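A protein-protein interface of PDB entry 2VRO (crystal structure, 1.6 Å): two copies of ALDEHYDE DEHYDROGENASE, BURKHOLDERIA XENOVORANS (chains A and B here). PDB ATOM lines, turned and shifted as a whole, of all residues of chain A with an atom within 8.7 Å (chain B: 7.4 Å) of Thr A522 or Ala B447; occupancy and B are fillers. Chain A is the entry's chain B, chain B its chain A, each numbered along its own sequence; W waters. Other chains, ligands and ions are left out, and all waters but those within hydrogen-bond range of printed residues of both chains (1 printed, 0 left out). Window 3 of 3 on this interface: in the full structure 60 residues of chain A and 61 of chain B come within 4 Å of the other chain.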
ATOM      1  N   ILE A 513      20.144 -37.097  21.613  1.00  0.00           N
ATOM      2  CA  ILE A 513      20.721 -36.049  20.794  1.00  0.00           C
ATOM      3  C   ILE A 513      21.592 -36.709  19.735  1.00  0.00           C
ATOM      4  O   ILE A 513      22.553 -37.400  20.069  1.00  0.00           O
ATOM      5  CB  ILE A 513      21.630 -35.094  21.595  1.00  0.00           C
ATOM      6  CG1 ILE A 513      21.003 -34.674  22.929  1.00  0.00           C
ATOM      7  CG2 ILE A 513      22.053 -33.916  20.703  1.00  0.00           C
ATOM      8  CD1 ILE A 513      19.752 -33.858  22.834  1.00  0.00           C
ATOM      9  N   ALA A 515      23.981 -35.977  16.430  1.00  0.00           N
ATOM     10  CA  ALA A 515      24.721 -34.815  15.930  1.00  0.00           C
ATOM     11  C   ALA A 515      26.147 -35.130  15.506  1.00  0.00           C
ATOM     12  O   ALA A 515      26.682 -36.207  15.791  1.00  0.00           O
ATOM     13  CB  ALA A 515      24.730 -33.706  16.987  1.00  0.00           C
ATOM     14  N   ALA A 516      26.763 -34.167  14.832  1.00  0.00           N
ATOM     15  CA  ALA A 516      28.203 -34.233  14.563  1.00  0.00           C
ATOM     16  C   ALA A 516      29.017 -34.418  15.864  1.00  0.00           C
ATOM     17  O   ALA A 516      28.616 -33.938  16.934  1.00  0.00           O
ATOM     18  CB  ALA A 516      28.632 -32.986  13.828  1.00  0.00           C
ATOM     19  N   SER A 517      30.160 -35.110  15.754  1.00  0.00           N
ATOM     20  CA  SER A 517      31.042 -35.390  16.901  1.00  0.00           C
ATOM     21  C   SER A 517      31.310 -34.169  17.788  1.00  0.00           C
ATOM     22  O   SER A 517      31.267 -34.278  19.009  1.00  0.00           O
ATOM     23  CB  SER A 517      32.395 -35.944  16.428  1.00  0.00           C
ATOM     24  OG  SER A 517      32.226 -37.090  15.611  1.00  0.00           O
ATOM     25  N   ALA A 518      31.628 -33.029  17.169  1.00  0.00           N
ATOM     26  CA  ALA A 518      31.977 -31.811  17.914  1.00  0.00           C
ATOM     27  C   ALA A 518      30.772 -31.269  18.692  1.00  0.00           C
ATOM     28  O   ALA A 518      30.920 -30.703  19.777  1.00  0.00           O
ATOM     29  CB  ALA A 518      32.536 -30.753  16.985  1.00  0.00           C
ATOM     30  N   ALA A 519      29.570 -31.468  18.146  1.00  0.00           N
ATOM     31  CA  ALA A 519      28.355 -31.067  18.852  1.00  0.00           C
ATOM     32  C   ALA A 519      28.122 -31.990  20.066  1.00  0.00           C
ATOM     33  O   ALA A 519      27.765 -31.522  21.157  1.00  0.00           O
ATOM     34  CB  ALA A 519      27.160 -31.066  17.908  1.00  0.00           C
ATOM     35  N   ILE A 520      28.314 -33.291  19.868  1.00  0.00           N
ATOM     36  CA  ILE A 520      28.254 -34.262  20.972  1.00  0.00           C
ATOM     37  C   ILE A 520      29.305 -33.922  22.046  1.00  0.00           C
ATOM     38  O   ILE A 520      29.012 -33.941  23.233  1.00  0.00           O
ATOM     39  CB  ILE A 520      28.422 -35.733  20.489  1.00  0.00           C
ATOM     40  CG1 ILE A 520      27.312 -36.136  19.490  1.00  0.00           C
ATOM     41  CG2 ILE A 520      28.510 -36.702  21.690  1.00  0.00           C
ATOM     42  CD1 ILE A 520      25.879 -36.071  20.064  1.00  0.00           C
ATOM     43  N   GLY A 521      30.517 -33.555  21.622  1.00  0.00           N
ATOM     44  CA  GLY A 521      31.545 -33.094  22.559  1.00  0.00           C
ATOM     45  C   GLY A 521      31.134 -31.919  23.437  1.00  0.00           C
ATOM     46  O   GLY A 521      31.393 -31.917  24.645  1.00  0.00           O
ATOM     47  N   THR A 522      30.498 -30.913  22.830  1.00  0.00           N
ATOM     48  CA  THR A 522      30.122 -29.690  23.548  1.00  0.00           C
ATOM     49  C   THR A 522      28.929 -29.929  24.465  1.00  0.00           C
ATOM     50  O   THR A 522      28.883 -29.413  25.590  1.00  0.00           O
ATOM     51  CB  THR A 522      29.859 -28.463  22.610  1.00  0.00           C
ATOM     52  OG1 THR A 522      28.664 -28.654  21.842  1.00  0.00           O
ATOM     53  CG2 THR A 522      31.025 -28.246  21.692  1.00  0.00           C
ATOM     54  N   LEU A 523      27.981 -30.749  24.016  1.00  0.00           N
ATOM     55  CA  LEU A 523      26.853 -31.056  24.893  1.00  0.00           C
ATOM     56  C   LEU A 523      27.320 -31.915  26.074  1.00  0.00           C
ATOM     57  O   LEU A 523      26.870 -31.716  27.197  1.00  0.00           O
ATOM     58  CB  LEU A 523      25.676 -31.655  24.123  1.00  0.00           C
ATOM     59  CG  LEU A 523      25.582 -33.115  23.740  1.00  0.00           C
ATOM     60  CD1 LEU A 523      24.793 -33.866  24.786  1.00  0.00           C
ATOM     61  CD2 LEU A 523      24.874 -33.186  22.419  1.00  0.00           C
ATOM     62  N   THR A 524      28.269 -32.812  25.817  1.00  0.00           N
ATOM     63  CA  THR A 524      28.850 -33.684  26.847  1.00  0.00           C
ATOM     64  C   THR A 524      29.614 -32.941  27.974  1.00  0.00           C
ATOM     65  O   THR A 524      29.500 -33.323  29.147  1.00  0.00           O
ATOM     66  CB  THR A 524      29.687 -34.819  26.200  1.00  0.00           C
ATOM     67  OG1 THR A 524      28.869 -35.528  25.259  1.00  0.00           O
ATOM     68  CG2 THR A 524      30.185 -35.809  27.234  1.00  0.00           C
ATOM     69  N   GLN A 525      30.359 -31.880  27.632  1.00  0.00           N
ATOM     70  CA  GLN A 525      31.011 -31.002  28.635  1.00  0.00           C
ATOM     71  C   GLN A 525      30.033 -30.412  29.646  1.00  0.00           C
ATOM     72  O   GLN A 525      30.449 -29.917  30.704  1.00  0.00           O
ATOM     73  CB  GLN A 525      31.679 -29.784  27.980  1.00  0.00           C
ATOM     74  CG  GLN A 525      32.636 -30.050  26.874  1.00  0.00           C
ATOM     75  CD  GLN A 525      33.370 -28.781  26.448  1.00  0.00           C
ATOM     76  OE1 GLN A 525      32.773 -27.705  26.347  1.00  0.00           O
ATOM     77  NE2 GLN A 525      34.673 -28.904  26.209  1.00  0.00           N
ATOM     78  N   ALA A 526      28.748 -30.416  29.281  1.00  0.00           N
ATOM     79  CA  ALA A 526      27.693 -29.781  30.064  1.00  0.00           C
ATOM     80  C   ALA A 526      26.852 -30.837  30.786  1.00  0.00           C
ATOM     81  O   ALA A 526      25.759 -30.553  31.287  1.00  0.00           O
ATOM     82  CB  ALA A 526      26.823 -28.909  29.163  1.00  0.00           C
ATOM     83  N   THR A 527      27.364 -32.063  30.802  1.00  0.00           N
ATOM     84  CA  THR A 527      26.709 -33.165  31.514  1.00  0.00           C
ATOM     85  C   THR A 527      27.661 -33.910  32.452  1.00  0.00           C
ATOM     86  O   THR A 527      28.878 -33.673  32.457  1.00  0.00           O
ATOM     87  CB  THR A 527      26.081 -34.172  30.548  1.00  0.00           C
ATOM     88  OG1 THR A 527      27.116 -34.823  29.796  1.00  0.00           O
ATOM     89  CG2 THR A 527      25.095 -33.479  29.595  1.00  0.00           C
ATOM     90  N   SER B 443      22.888 -25.698  11.270  1.00  0.00           N
ATOM     91  CA  SER B 443      23.951 -24.688  11.473  1.00  0.00           C
ATOM     92  C   SER B 443      25.225 -25.103  10.749  1.00  0.00           C
ATOM     93  O   SER B 443      25.421 -26.277  10.465  1.00  0.00           O
ATOM     94  CB  SER B 443      24.241 -24.539  12.968  1.00  0.00           C
ATOM     95  OG  SER B 443      25.215 -23.537  13.239  1.00  0.00           O
ATOM     96  N   ASN B 444      26.092 -24.129  10.443  1.00  0.00           N
ATOM     97  CA  ASN B 444      27.464 -24.423  10.000  1.00  0.00           C
ATOM     98  C   ASN B 444      28.403 -24.705  11.175  1.00  0.00           C
ATOM     99  O   ASN B 444      29.514 -25.216  10.984  1.00  0.00           O
ATOM    100  CB  ASN B 444      28.010 -23.264   9.152  1.00  0.00           C
ATOM    101  CG  ASN B 444      27.072 -22.885   8.017  1.00  0.00           C
ATOM    102  OD1 ASN B 444      27.009 -23.562   6.991  1.00  0.00           O
ATOM    103  ND2 ASN B 444      26.332 -21.808   8.209  1.00  0.00           N
ATOM    104  N   ASP B 445      27.917 -24.406  12.381  1.00  0.00           N
ATOM    105  CA  ASP B 445      28.708 -24.392  13.616  1.00  0.00           C
ATOM    106  C   ASP B 445      28.312 -25.569  14.516  1.00  0.00           C
ATOM    107  O   ASP B 445      27.351 -25.473  15.286  1.00  0.00           O
ATOM    108  CB  ASP B 445      28.464 -23.047  14.332  1.00  0.00           C
ATOM    109  CG  ASP B 445      29.330 -22.847  15.581  1.00  0.00           C
ATOM    110  OD1 ASP B 445      29.983 -23.807  16.053  1.00  0.00           O
ATOM    111  OD2 ASP B 445      29.329 -21.704  16.103  1.00  0.00           O
ATOM    112  N   ASP B 446      29.077 -26.658  14.420  1.00  0.00           N
ATOM    113  CA  ASP B 446      28.817 -27.897  15.183  1.00  0.00           C
ATOM    114  C   ASP B 446      28.743 -27.677  16.697  1.00  0.00           C
ATOM    115  O   ASP B 446      27.844 -28.205  17.369  1.00  0.00           O
ATOM    116  CB  ASP B 446      29.867 -28.966  14.846  1.00  0.00           C
ATOM    117  CG  ASP B 446      29.726 -29.507  13.423  1.00  0.00           C
ATOM    118  OD1 ASP B 446      28.819 -29.062  12.696  1.00  0.00           O
ATOM    119  OD2 ASP B 446      30.520 -30.382  13.027  1.00  0.00           O
ATOM    120  N   ALA B 447      29.677 -26.887  17.232  1.00  0.00           N
ATOM    121  CA  ALA B 447      29.708 -26.602  18.661  1.00  0.00           C
ATOM    122  C   ALA B 447      28.430 -25.927  19.137  1.00  0.00           C
ATOM    123  O   ALA B 447      27.884 -26.296  20.182  1.00  0.00           O
ATOM    124  CB  ALA B 447      30.935 -25.761  19.021  1.00  0.00           C
ATOM    125  N   HIS B 448      27.953 -24.952  18.362  1.00  0.00           N
ATOM    126  CA  HIS B 448      26.736 -24.219  18.686  1.00  0.00           C
ATOM    127  C   HIS B 448      25.544 -25.175  18.758  1.00  0.00           C
ATOM    128  O   HIS B 448      24.679 -25.040  19.634  1.00  0.00           O
ATOM    129  CB  HIS B 448      26.484 -23.106  17.657  1.00  0.00           C
ATOM    130  CG  HIS B 448      25.300 -22.251  17.972  1.00  0.00           C
ATOM    131  ND1 HIS B 448      25.290 -21.348  19.015  1.00  0.00           N
ATOM    132  CD2 HIS B 448      24.086 -22.156  17.379  1.00  0.00           C
ATOM    133  CE1 HIS B 448      24.115 -20.744  19.057  1.00  0.00           C
ATOM    134  NE2 HIS B 448      23.371 -21.212  18.072  1.00  0.00           N
ATOM    135  N   LEU B 449      25.525 -26.154  17.852  1.00  0.00           N
ATOM    136  CA  LEU B 449      24.430 -27.125  17.800  1.00  0.00           C
ATOM    137  C   LEU B 449      24.309 -27.934  19.096  1.00  0.00           C
ATOM    138  O   LEU B 449      23.203 -28.148  19.573  1.00  0.00           O
ATOM    139  CB  LEU B 449      24.549 -28.047  16.579  1.00  0.00           C
ATOM    140  CG  LEU B 449      24.272 -27.411  15.208  1.00  0.00           C
ATOM    141  CD1 LEU B 449      24.637 -28.378  14.086  1.00  0.00           C
ATOM    142  CD2 LEU B 449      22.798 -26.968  15.080  1.00  0.00           C
ATOM    143  N   GLY B 450      25.445 -28.340  19.665  1.00  0.00           N
ATOM    144  CA  GLY B 450      25.476 -29.045  20.958  1.00  0.00           C
ATOM    145  C   GLY B 450      24.809 -28.248  22.071  1.00  0.00           C
ATOM    146  O   GLY B 450      23.995 -28.777  22.830  1.00  0.00           O
ATOM    147  N   ARG B 451      25.145 -26.962  22.152  1.00  0.00           N
ATOM    148  CA  ARG B 451      24.518 -26.039  23.106  1.00  0.00           C
ATOM    149  C   ARG B 451      23.024 -25.854  22.878  1.00  0.00           C
ATOM    150  O   ARG B 451      22.236 -25.920  23.828  1.00  0.00           O
ATOM    151  CB  ARG B 451      25.216 -24.673  23.062  1.00  0.00           C
ATOM    152  CG  ARG B 451      26.544 -24.648  23.801  1.00  0.00           C
ATOM    153  CD  ARG B 451      27.263 -23.294  23.672  1.00  0.00           C
ATOM    154  NE  ARG B 451      28.176 -23.289  22.524  1.00  0.00           N
ATOM    155  CZ  ARG B 451      28.107 -22.449  21.492  1.00  0.00           C
ATOM    156  NH1 ARG B 451      27.176 -21.498  21.444  1.00  0.00           N
ATOM    157  NH2 ARG B 451      28.992 -22.552  20.507  1.00  0.00           N
ATOM    158  N   LEU B 452      22.634 -25.607  21.626  1.00  0.00           N
ATOM    159  CA  LEU B 452      21.210 -25.435  21.286  1.00  0.00           C
ATOM    160  C   LEU B 452      20.413 -26.710  21.559  1.00  0.00           C
ATOM    161  O   LEU B 452      19.291 -26.641  22.051  1.00  0.00           O
ATOM    162  CB  LEU B 452      21.034 -24.991  19.823  1.00  0.00           C
ATOM    163  CG  LEU B 452      19.628 -24.737  19.253  1.00  0.00           C
ATOM    164  CD1 LEU B 452      18.829 -23.728  20.056  1.00  0.00           C
ATOM    165  CD2 LEU B 452      19.726 -24.320  17.785  1.00  0.00           C
ATOM    166  N   ALA B 453      21.013 -27.860  21.253  1.00  0.00           N
ATOM    167  CA  ALA B 453      20.358 -29.148  21.479  1.00  0.00           C
ATOM    168  C   ALA B 453      19.912 -29.300  22.938  1.00  0.00           C
ATOM    169  O   ALA B 453      18.782 -29.744  23.217  1.00  0.00           O
ATOM    170  CB  ALA B 453      21.277 -30.299  21.075  1.00  0.00           C
ATOM    171  N   LEU B 454      20.796 -28.929  23.872  1.00  0.00           N
ATOM    172  CA  LEU B 454      20.490 -29.037  25.297  1.00  0.00           C
ATOM    173  C   LEU B 454      19.318 -28.148  25.683  1.00  0.00           C
ATOM    174  O   LEU B 454      18.572 -28.454  26.604  1.00  0.00           O
ATOM    175  CB  LEU B 454      21.717 -28.722  26.163  1.00  0.00           C
ATOM    176  CG  LEU B 454      22.787 -29.815  26.238  1.00  0.00           C
ATOM    177  CD1 LEU B 454      24.000 -29.279  26.950  1.00  0.00           C
ATOM    178  CD2 LEU B 454      22.288 -31.100  26.921  1.00  0.00           C
HETATM  179  O   HOH W   1      32.238 -32.789  14.388  1.00  0.00           O
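Water W1 lies within hydrogen-bond range of N of Ala A518 (2.9 Å), OD2 of Asp B446 (3.3 Å) and N of Ser A517 (3.4 Å).
Of the printed residues of chain B, Ile A513 touches Ala B453.
Of the printed residues of chain B, Ala A516 touches Asp B446.
Ile A520 touches none of the printed residues of chain B.
Of chain B, only Ala B447, Gly B450 and Arg B451 come within 4 Å of Thr A522.
Printed residues of chain A within 4 Å of Ala B447: Thr A522 (3.0 Å).
Leu B452 touches none of the printed residues of chain A.
Of the printed residues of chain A, Leu B454 touches Leu A523 (3.8 Å) and Ala A526 (3.6 Å).
The nearest residue of chain A that does not touch Ala B447 is Ala A518 (4.4 Å).
OG1 of Thr A522 lies within hydrogen-bond range of O of Ala B447 (3.0 Å).
ND1 of His B448 lies within hydrogen-bond range of NH1 of Arg B451, 3.1 Å away.
The backbone carbonyl oxygen (O) of Ala A519 lies within hydrogen-bond range of the side-chain hydroxyl (OG1) of Thr A522.
The side-chain carboxylate (OD1) of Asp B445 sits at hydrogen-bond distance from the backbone NH (N) of Ala B447, 3.3 Å away.
No position is printed for both chains.
Of the 11 pairs that touch across the chains among the printed residues, none has its exchanged pair printed and touching as well.
Ile A513 touches Ala B453.
Ala A516 touches Asp B446.
CB of Ala A518 touches CB of Asp B446 (3.9 Å).
Ala A519 touches Asp B446 (CB to O, 3.0 Å).
Ala A519 touches Gly B450.
Thr A522 touches Gly B450 (OG1 to CA, 3.3 Å).
Arg B451 touches Thr A522.
Leu A523 touches Gly B450 (CB to O, 3.6 Å).
Leu B454 touches Leu A523.
Ala A526 touches Leu B454 (CB to CD1, 3.6 Å).
Printed residues of chain A that touch a printed residue of chain B: Ile A513, Ala A516, Ala A518, Ala A519, Thr A522, Leu A523 and Ala A526.
Hydrophobic or aromatic side chains of chain A within 4 Å of the printed part of chain B: Ile A513, Ala A516, Ala A518, Ala A519, Leu A523 and Ala A526.
Among the printed residues, 11 pairs touch across the chains.
Among the printed residues, no Asp or Glu carboxylate lies within 4 Å of a Lys or Arg side-chain nitrogen of the other chain.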
